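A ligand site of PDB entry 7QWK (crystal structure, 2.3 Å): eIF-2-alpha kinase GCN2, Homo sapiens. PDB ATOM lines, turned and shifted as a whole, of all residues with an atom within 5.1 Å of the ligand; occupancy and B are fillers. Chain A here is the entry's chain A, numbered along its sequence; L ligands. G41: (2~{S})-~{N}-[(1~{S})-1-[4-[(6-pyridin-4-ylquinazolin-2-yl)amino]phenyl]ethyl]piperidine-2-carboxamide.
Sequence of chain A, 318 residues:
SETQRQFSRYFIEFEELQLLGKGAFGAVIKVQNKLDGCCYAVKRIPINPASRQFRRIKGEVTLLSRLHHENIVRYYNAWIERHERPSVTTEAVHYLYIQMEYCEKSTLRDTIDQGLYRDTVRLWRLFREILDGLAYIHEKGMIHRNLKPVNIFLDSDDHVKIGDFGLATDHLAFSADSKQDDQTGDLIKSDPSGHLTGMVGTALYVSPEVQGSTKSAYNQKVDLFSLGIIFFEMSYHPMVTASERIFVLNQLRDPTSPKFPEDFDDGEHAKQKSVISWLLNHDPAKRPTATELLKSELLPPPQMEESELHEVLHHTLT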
ATOM      1  N   GLN A  18     -10.350   8.033  -0.449  1.00  0.00           N
ATOM      2  CA  GLN A  18     -11.370   8.224   0.554  1.00  0.00           C
ATOM      3  C   GLN A  18     -10.750   8.775   1.798  1.00  0.00           C
ATOM      4  O   GLN A  18      -9.627   8.388   2.137  1.00  0.00           O
ATOM      5  CB  GLN A  18     -11.959   6.830   0.890  1.00  0.00           C
ATOM      6  CG  GLN A  18     -13.385   6.829   1.421  1.00  0.00           C
ATOM      7  CD  GLN A  18     -13.771   5.465   1.923  1.00  0.00           C
ATOM      8  OE1 GLN A  18     -13.302   4.441   1.407  1.00  0.00           O
ATOM      9  NE2 GLN A  18     -14.611   5.421   2.951  1.00  0.00           N
ATOM     10  N   LEU A  20     -10.469   8.605   5.559  1.00  0.00           N
ATOM     11  CA  LEU A  20     -10.721   7.620   6.601  1.00  0.00           C
ATOM     12  C   LEU A  20     -10.917   8.296   7.942  1.00  0.00           C
ATOM     13  O   LEU A  20     -11.643   7.802   8.797  1.00  0.00           O
ATOM     14  CB  LEU A  20      -9.554   6.637   6.687  1.00  0.00           C
ATOM     15  CG  LEU A  20      -9.195   5.898   5.370  1.00  0.00           C
ATOM     16  CD1 LEU A  20      -7.886   5.165   5.486  1.00  0.00           C
ATOM     17  CD2 LEU A  20     -10.321   4.975   4.891  1.00  0.00           C
ATOM     18  N   VAL A  28      -6.527  11.208   8.000  1.00  0.00           N
ATOM     19  CA  VAL A  28      -6.041   9.936   7.453  1.00  0.00           C
ATOM     20  C   VAL A  28      -6.788   9.741   6.155  1.00  0.00           C
ATOM     21  O   VAL A  28      -8.005   9.878   6.125  1.00  0.00           O
ATOM     22  CB  VAL A  28      -6.238   8.722   8.424  1.00  0.00           C
ATOM     23  CG1 VAL A  28      -5.561   7.467   7.884  1.00  0.00           C
ATOM     24  CG2 VAL A  28      -5.708   9.045   9.816  1.00  0.00           C
ATOM     25  N   ALA A  41      -2.988   3.709   3.828  1.00  0.00           N
ATOM     26  CA  ALA A  41      -3.587   4.698   4.741  1.00  0.00           C
ATOM     27  C   ALA A  41      -2.462   5.740   5.004  1.00  0.00           C
ATOM     28  O   ALA A  41      -1.380   5.383   5.509  1.00  0.00           O
ATOM     29  CB  ALA A  41      -4.005   4.041   6.040  1.00  0.00           C
ATOM     30  N   LYS A  43      -1.571   9.176   6.860  1.00  0.00           N
ATOM     31  CA  LYS A  43      -1.882  10.106   7.943  1.00  0.00           C
ATOM     32  C   LYS A  43      -1.148  11.409   7.646  1.00  0.00           C
ATOM     33  O   LYS A  43       0.035  11.374   7.345  1.00  0.00           O
ATOM     34  CB  LYS A  43      -1.378   9.532   9.261  1.00  0.00           C
ATOM     35  CG  LYS A  43      -1.928  10.221  10.492  1.00  0.00           C
ATOM     36  CD  LYS A  43      -1.037   9.933  11.689  1.00  0.00           C
ATOM     37  CE  LYS A  43      -1.559  10.502  12.994  1.00  0.00           C
ATOM     38  NZ  LYS A  43      -1.031   9.733  14.170  1.00  0.00           N
ATOM     39  N   LEU A  64       8.479   3.908  15.547  1.00  0.00           N
ATOM     40  CA  LEU A  64       7.520   3.331  14.603  1.00  0.00           C
ATOM     41  C   LEU A  64       8.252   2.671  13.434  1.00  0.00           C
ATOM     42  O   LEU A  64       7.944   1.541  13.082  1.00  0.00           O
ATOM     43  CB  LEU A  64       6.648   4.503  14.068  1.00  0.00           C
ATOM     44  CG  LEU A  64       5.466   4.187  13.174  1.00  0.00           C
ATOM     45  CD1 LEU A  64       4.240   3.848  14.005  1.00  0.00           C
ATOM     46  CD2 LEU A  64       5.123   5.377  12.333  1.00  0.00           C
ATOM     47  N   VAL A  73       0.628  -2.638  12.461  1.00  0.00           N
ATOM     48  CA  VAL A  73       0.380  -2.081  11.128  1.00  0.00           C
ATOM     49  C   VAL A  73       1.741  -1.745  10.478  1.00  0.00           C
ATOM     50  O   VAL A  73       2.556  -1.045  11.085  1.00  0.00           O
ATOM     51  CB  VAL A  73      -0.668  -0.938  11.064  1.00  0.00           C
ATOM     52  CG1 VAL A  73      -0.393   0.121  12.108  1.00  0.00           C
ATOM     53  CG2 VAL A  73      -0.728  -0.285   9.691  1.00  0.00           C
ATOM     54  N   ILE A  98       2.649  10.163   6.977  1.00  0.00           N
ATOM     55  CA  ILE A  98       3.055   8.816   7.414  1.00  0.00           C
ATOM     56  C   ILE A  98       2.236   7.847   6.571  1.00  0.00           C
ATOM     57  O   ILE A  98       1.018   7.816   6.715  1.00  0.00           O
ATOM     58  CB  ILE A  98       2.861   8.544   8.953  1.00  0.00           C
ATOM     59  CG1 ILE A  98       3.450   9.666   9.846  1.00  0.00           C
ATOM     60  CG2 ILE A  98       3.482   7.187   9.350  1.00  0.00           C
ATOM     61  CD1 ILE A  98       2.834   9.739  11.172  1.00  0.00           C
ATOM     62  N   MET A 100       1.167   4.117   5.796  1.00  0.00           N
ATOM     63  CA  MET A 100       1.065   2.808   6.484  1.00  0.00           C
ATOM     64  C   MET A 100       0.356   1.795   5.618  1.00  0.00           C
ATOM     65  O   MET A 100      -0.152   2.156   4.550  1.00  0.00           O
ATOM     66  CB  MET A 100       0.251   2.969   7.800  1.00  0.00           C
ATOM     67  CG  MET A 100       0.798   4.016   8.761  1.00  0.00           C
ATOM     68  SD  MET A 100       2.476   3.614   9.326  1.00  0.00           S
ATOM     69  CE  MET A 100       2.145   2.476  10.621  1.00  0.00           C
ATOM     70  N   GLU A 101       0.237   0.530   6.070  1.00  0.00           N
ATOM     71  CA  GLU A 101      -0.590  -0.405   5.313  1.00  0.00           C
ATOM     72  C   GLU A 101      -2.053  -0.030   5.522  1.00  0.00           C
ATOM     73  O   GLU A 101      -2.441   0.510   6.564  1.00  0.00           O
ATOM     74  CB  GLU A 101      -0.348  -1.890   5.711  1.00  0.00           C
ATOM     75  CG  GLU A 101      -1.222  -2.446   6.816  1.00  0.00           C
ATOM     76  CD  GLU A 101      -0.913  -3.839   7.321  1.00  0.00           C
ATOM     77  OE1 GLU A 101      -1.612  -4.780   6.899  1.00  0.00           O
ATOM     78  OE2 GLU A 101       0.000  -3.986   8.167  1.00  0.00           O
ATOM     79  N   TYR A 102      -2.849  -0.324   4.523  1.00  0.00           N
ATOM     80  CA  TYR A 102      -4.280  -0.128   4.577  1.00  0.00           C
ATOM     81  C   TYR A 102      -4.877  -1.484   4.981  1.00  0.00           C
ATOM     82  O   TYR A 102      -4.676  -2.479   4.296  1.00  0.00           O
ATOM     83  CB  TYR A 102      -4.826   0.336   3.208  1.00  0.00           C
ATOM     84  CG  TYR A 102      -6.328   0.463   3.213  1.00  0.00           C
ATOM     85  CD1 TYR A 102      -6.968   1.456   3.955  1.00  0.00           C
ATOM     86  CD2 TYR A 102      -7.118  -0.488   2.569  1.00  0.00           C
ATOM     87  CE1 TYR A 102      -8.364   1.486   4.072  1.00  0.00           C
ATOM     88  CE2 TYR A 102      -8.512  -0.463   2.673  1.00  0.00           C
ATOM     89  CZ  TYR A 102      -9.130   0.539   3.408  1.00  0.00           C
ATOM     90  OH  TYR A 102     -10.507   0.584   3.422  1.00  0.00           O
ATOM     91  N   CYS A 103      -5.558  -1.513   6.149  1.00  0.00           N
ATOM     92  CA  CYS A 103      -6.226  -2.691   6.687  1.00  0.00           C
ATOM     93  C   CYS A 103      -7.689  -2.726   6.200  1.00  0.00           C
ATOM     94  O   CYS A 103      -8.503  -1.901   6.589  1.00  0.00           O
ATOM     95  CB  CYS A 103      -6.102  -2.687   8.203  1.00  0.00           C
ATOM     96  SG  CYS A 103      -4.384  -2.874   8.785  1.00  0.00           S
ATOM     97  N   GLU A 104      -7.978  -3.664   5.300  1.00  0.00           N
ATOM     98  CA  GLU A 104      -9.243  -3.800   4.574  1.00  0.00           C
ATOM     99  C   GLU A 104     -10.479  -4.028   5.468  1.00  0.00           C
ATOM    100  O   GLU A 104     -11.540  -3.516   5.130  1.00  0.00           O
ATOM    101  CB  GLU A 104      -9.129  -4.884   3.499  1.00  0.00           C
ATOM    102  CG  GLU A 104      -7.807  -4.827   2.726  1.00  0.00           C
ATOM    103  CD  GLU A 104      -6.652  -5.740   3.152  1.00  0.00           C
ATOM    104  OE1 GLU A 104      -6.331  -5.828   4.371  1.00  0.00           O
ATOM    105  OE2 GLU A 104      -6.055  -6.360   2.242  1.00  0.00           O
ATOM    106  N   SER A 106     -11.228  -2.836   8.391  1.00  0.00           N
ATOM    107  CA  SER A 106     -11.279  -1.692   9.309  1.00  0.00           C
ATOM    108  C   SER A 106     -10.723  -1.952  10.724  1.00  0.00           C
ATOM    109  O   SER A 106      -9.627  -2.499  10.835  1.00  0.00           O
ATOM    110  CB  SER A 106     -12.687  -1.077   9.351  1.00  0.00           C
ATOM    111  OG  SER A 106     -13.647  -1.981   9.851  1.00  0.00           O
ATOM    112  N   THR A 107     -11.397  -1.468  11.795  1.00  0.00           N
ATOM    113  CA  THR A 107     -10.892  -1.477  13.173  1.00  0.00           C
ATOM    114  C   THR A 107     -11.565  -2.486  14.106  1.00  0.00           C
ATOM    115  O   THR A 107     -12.662  -2.951  13.793  1.00  0.00           O
ATOM    116  CB  THR A 107     -11.026  -0.067  13.802  1.00  0.00           C
ATOM    117  OG1 THR A 107     -12.402   0.205  14.006  1.00  0.00           O
ATOM    118  CG2 THR A 107     -10.461   1.013  12.959  1.00  0.00           C
ATOM    119  N   ARG A 109     -13.063  -1.720  16.821  1.00  0.00           N
ATOM    120  CA  ARG A 109     -14.304  -1.114  17.291  1.00  0.00           C
ATOM    121  C   ARG A 109     -15.486  -1.667  16.480  1.00  0.00           C
ATOM    122  O   ARG A 109     -16.444  -2.194  17.058  1.00  0.00           O
ATOM    123  CB  ARG A 109     -14.237   0.426  17.262  1.00  0.00           C
ATOM    124  CG  ARG A 109     -15.554   1.165  17.565  1.00  0.00           C
ATOM    125  CD  ARG A 109     -16.310   0.686  18.786  1.00  0.00           C
ATOM    126  NE  ARG A 109     -15.630   1.067  20.022  1.00  0.00           N
ATOM    127  CZ  ARG A 109     -15.640   0.345  21.131  1.00  0.00           C
ATOM    128  NH1 ARG A 109     -16.300  -0.817  21.172  1.00  0.00           N
ATOM    129  NH2 ARG A 109     -14.984   0.753  22.199  1.00  0.00           N
ATOM    130  N   ASP A 110     -15.339  -1.682  15.151  1.00  0.00           N
ATOM    131  CA  ASP A 110     -16.297  -2.201  14.193  1.00  0.00           C
ATOM    132  C   ASP A 110     -16.647  -3.654  14.466  1.00  0.00           C
ATOM    133  O   ASP A 110     -17.832  -3.983  14.454  1.00  0.00           O
ATOM    134  CB  ASP A 110     -15.776  -2.023  12.783  1.00  0.00           C
ATOM    135  CG  ASP A 110     -15.397  -0.584  12.467  1.00  0.00           C
ATOM    136  OD1 ASP A 110     -16.258   0.309  12.658  1.00  0.00           O
ATOM    137  OD2 ASP A 110     -14.246  -0.345  12.076  1.00  0.00           O
ATOM    138  N   VAL A 150     -10.433   1.411  18.424  1.00  0.00           N
ATOM    139  CA  VAL A 150     -10.356   2.202  17.177  1.00  0.00           C
ATOM    140  C   VAL A 150      -8.916   2.249  16.600  1.00  0.00           C
ATOM    141  O   VAL A 150      -8.736   2.533  15.416  1.00  0.00           O
ATOM    142  CB  VAL A 150     -10.948   3.626  17.291  1.00  0.00           C
ATOM    143  CG1 VAL A 150     -12.423   3.590  17.635  1.00  0.00           C
ATOM    144  CG2 VAL A 150     -10.166   4.515  18.266  1.00  0.00           C
ATOM    145  N   PHE A 153      -6.458  -2.484  14.148  1.00  0.00           N
ATOM    146  CA  PHE A 153      -7.075  -2.749  12.863  1.00  0.00           C
ATOM    147  C   PHE A 153      -7.106  -4.223  12.512  1.00  0.00           C
ATOM    148  O   PHE A 153      -6.367  -5.020  13.068  1.00  0.00           O
ATOM    149  CB  PHE A 153      -6.382  -1.917  11.755  1.00  0.00           C
ATOM    150  CG  PHE A 153      -6.257  -0.461  12.124  1.00  0.00           C
ATOM    151  CD1 PHE A 153      -5.243  -0.012  12.951  1.00  0.00           C
ATOM    152  CD2 PHE A 153      -7.158   0.472  11.615  1.00  0.00           C
ATOM    153  CE1 PHE A 153      -5.161   1.334  13.323  1.00  0.00           C
ATOM    154  CE2 PHE A 153      -7.077   1.813  12.004  1.00  0.00           C
ATOM    155  CZ  PHE A 153      -6.100   2.223  12.877  1.00  0.00           C
ATOM    156  N   GLY A 163      -2.242  -0.129  15.620  1.00  0.00           N
ATOM    157  CA  GLY A 163      -1.911   1.127  14.942  1.00  0.00           C
ATOM    158  C   GLY A 163      -2.072   2.370  15.778  1.00  0.00           C
ATOM    159  O   GLY A 163      -1.961   2.294  16.990  1.00  0.00           O
ATOM    160  N   ASP A 164      -2.375   3.529  15.148  1.00  0.00           N
ATOM    161  CA  ASP A 164      -2.469   4.800  15.878  1.00  0.00           C
ATOM    162  C   ASP A 164      -3.816   5.558  15.807  1.00  0.00           C
ATOM    163  O   ASP A 164      -4.209   6.062  16.869  1.00  0.00           O
ATOM    164  CB  ASP A 164      -1.345   5.741  15.464  1.00  0.00           C
ATOM    165  N   PHE A 165      -4.453   5.734  14.601  1.00  0.00           N
ATOM    166  CA  PHE A 165      -5.728   6.474  14.335  1.00  0.00           C
ATOM    167  C   PHE A 165      -5.968   7.740  15.193  1.00  0.00           C
ATOM    168  O   PHE A 165      -7.114   8.128  15.396  1.00  0.00           O
ATOM    169  CB  PHE A 165      -6.989   5.558  14.413  1.00  0.00           C
ATOM    170  CG  PHE A 165      -7.985   5.671  13.257  1.00  0.00           C
ATOM    171  CD1 PHE A 165      -8.066   6.824  12.486  1.00  0.00           C
ATOM    172  CD2 PHE A 165      -8.835   4.613  12.951  1.00  0.00           C
ATOM    173  CE1 PHE A 165      -8.953   6.902  11.411  1.00  0.00           C
ATOM    174  CE2 PHE A 165      -9.714   4.689  11.869  1.00  0.00           C
ATOM    175  CZ  PHE A 165      -9.775   5.839  11.112  1.00  0.00           C
HETATM  176  C1  G41 L   1     -13.671   2.903   7.246  1.00  0.00           C
HETATM  177  C2  G41 L   1     -12.259   2.378   7.293  1.00  0.00           C
HETATM  178  C3  G41 L   1     -11.256   3.066   7.964  1.00  0.00           C
HETATM  179  C7  G41 L   1     -11.924   1.189   6.662  1.00  0.00           C
HETATM  180  C8  G41 L   1      -7.190   1.336   7.971  1.00  0.00           C
HETATM  181  C9  G41 L   1      -4.992   0.985   8.315  1.00  0.00           C
HETATM  182  C10 G41 L   1      -4.863   2.185   9.068  1.00  0.00           C
HETATM  183  C11 G41 L   1      -3.699   2.700   9.682  1.00  0.00           C
HETATM  184  C12 G41 L   1      -3.705   3.890  10.383  1.00  0.00           C
HETATM  185  C13 G41 L   1      -4.911   4.585  10.501  1.00  0.00           C
HETATM  186  C14 G41 L   1      -6.059   4.122   9.932  1.00  0.00           C
HETATM  187  C15 G41 L   1      -6.068   2.916   9.196  1.00  0.00           C
HETATM  188  C16 G41 L   1      -2.470   4.387  11.017  1.00  0.00           C
HETATM  189  C19 G41 L   1      -0.878   6.119  11.448  1.00  0.00           C
HETATM  190  C20 G41 L   1      -2.040   5.698  10.829  1.00  0.00           C
HETATM  191  C21 G41 L   1     -14.531   2.641   9.533  1.00  0.00           C
HETATM  192  C22 G41 L   1     -14.905   3.341  10.839  1.00  0.00           C
HETATM  193  C24 G41 L   1     -14.094   4.280  13.031  1.00  0.00           C
HETATM  194  O   G41 L   1     -14.619   1.428   9.440  1.00  0.00           O
HETATM  195  N5  G41 L   1     -15.969   2.644  11.578  1.00  0.00           N
HETATM  196  C26 G41 L   1     -16.393   3.408  12.757  1.00  0.00           C
HETATM  197  C25 G41 L   1     -15.252   3.587  13.720  1.00  0.00           C
HETATM  198  C23 G41 L   1     -13.697   3.557  11.746  1.00  0.00           C
HETATM  199  N4  G41 L   1     -14.108   3.434   8.544  1.00  0.00           N
HETATM  200  C   G41 L   1     -13.841   3.987   6.186  1.00  0.00           C
HETATM  201  C6  G41 L   1     -10.631   0.696   6.705  1.00  0.00           C
HETATM  202  C5  G41 L   1      -9.637   1.394   7.377  1.00  0.00           C
HETATM  203  C4  G41 L   1      -9.958   2.585   8.010  1.00  0.00           C
HETATM  204  N   G41 L   1      -8.339   0.882   7.398  1.00  0.00           N
HETATM  205  N2  G41 L   1      -7.245   2.490   8.645  1.00  0.00           N
HETATM  206  N1  G41 L   1      -6.114   0.566   7.772  1.00  0.00           N
HETATM  207  N3  G41 L   1      -0.140   5.345  12.250  1.00  0.00           N
HETATM  208  C18 G41 L   1      -0.555   4.095  12.424  1.00  0.00           C
HETATM  209  C17 G41 L   1      -1.695   3.584  11.844  1.00  0.00           C
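OD2 of Asp 110 lies within hydrogen-bond range of OG of Ser 106, 2.8 Å away. OD2 of Asp 110 lies within hydrogen-bond range of OG1 of Thr 107 (2.7 Å). The backbone NH of Met 100 lies within hydrogen-bond range of the backbone carbonyl oxygen of Ala 41, at 2.9 Å. O of Val 28 sits at hydrogen-bond distance from N of Leu 20, at 2.8 Å. The backbone NH of Ile 98 sits at hydrogen-bond distance from the backbone carbonyl oxygen of Lys 43.
Residues that only touch the ligand: Glu 101 (3.1 Å), Ser 106 (3.2 Å), Phe 153 (3.2 Å), Tyr 102 (3.3 Å), Asp 164 (3.3 Å), Gln 18 (3.6 Å), Met 100 (3.6 Å), Ala 41 (3.7 Å), Val 73 (3.7 Å), Leu 20 (3.7 Å), Lys 43 (3.8 Å), Val 28 (3.9 Å) and Gly 163 (3.96 Å). Hydrophobic or aromatic side chains that line the ligand: Leu 20, Val 28, Ala 41, Val 73, Met 100, Tyr 102 and Phe 153. Within 4 Å of the ligand: Gln 18, Leu 20, Val 28, Ala 41, Lys 43, Val 73, Met 100, Glu 101, Tyr 102, Cys 103, Ser 106, Asp 110, Phe 153, Gly 163 and Asp 164.
A nitrogen (N5) of the ligand lies within salt-bridge range of the side-chain carboxylate (OD1) of Asp 110 (2.6 Å). N1 of the ligand sits at hydrogen-bond distance from N of Cys 103 (2.7 Å). N of the ligand lies within hydrogen-bond range of O of Cys 103 (2.9 Å).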
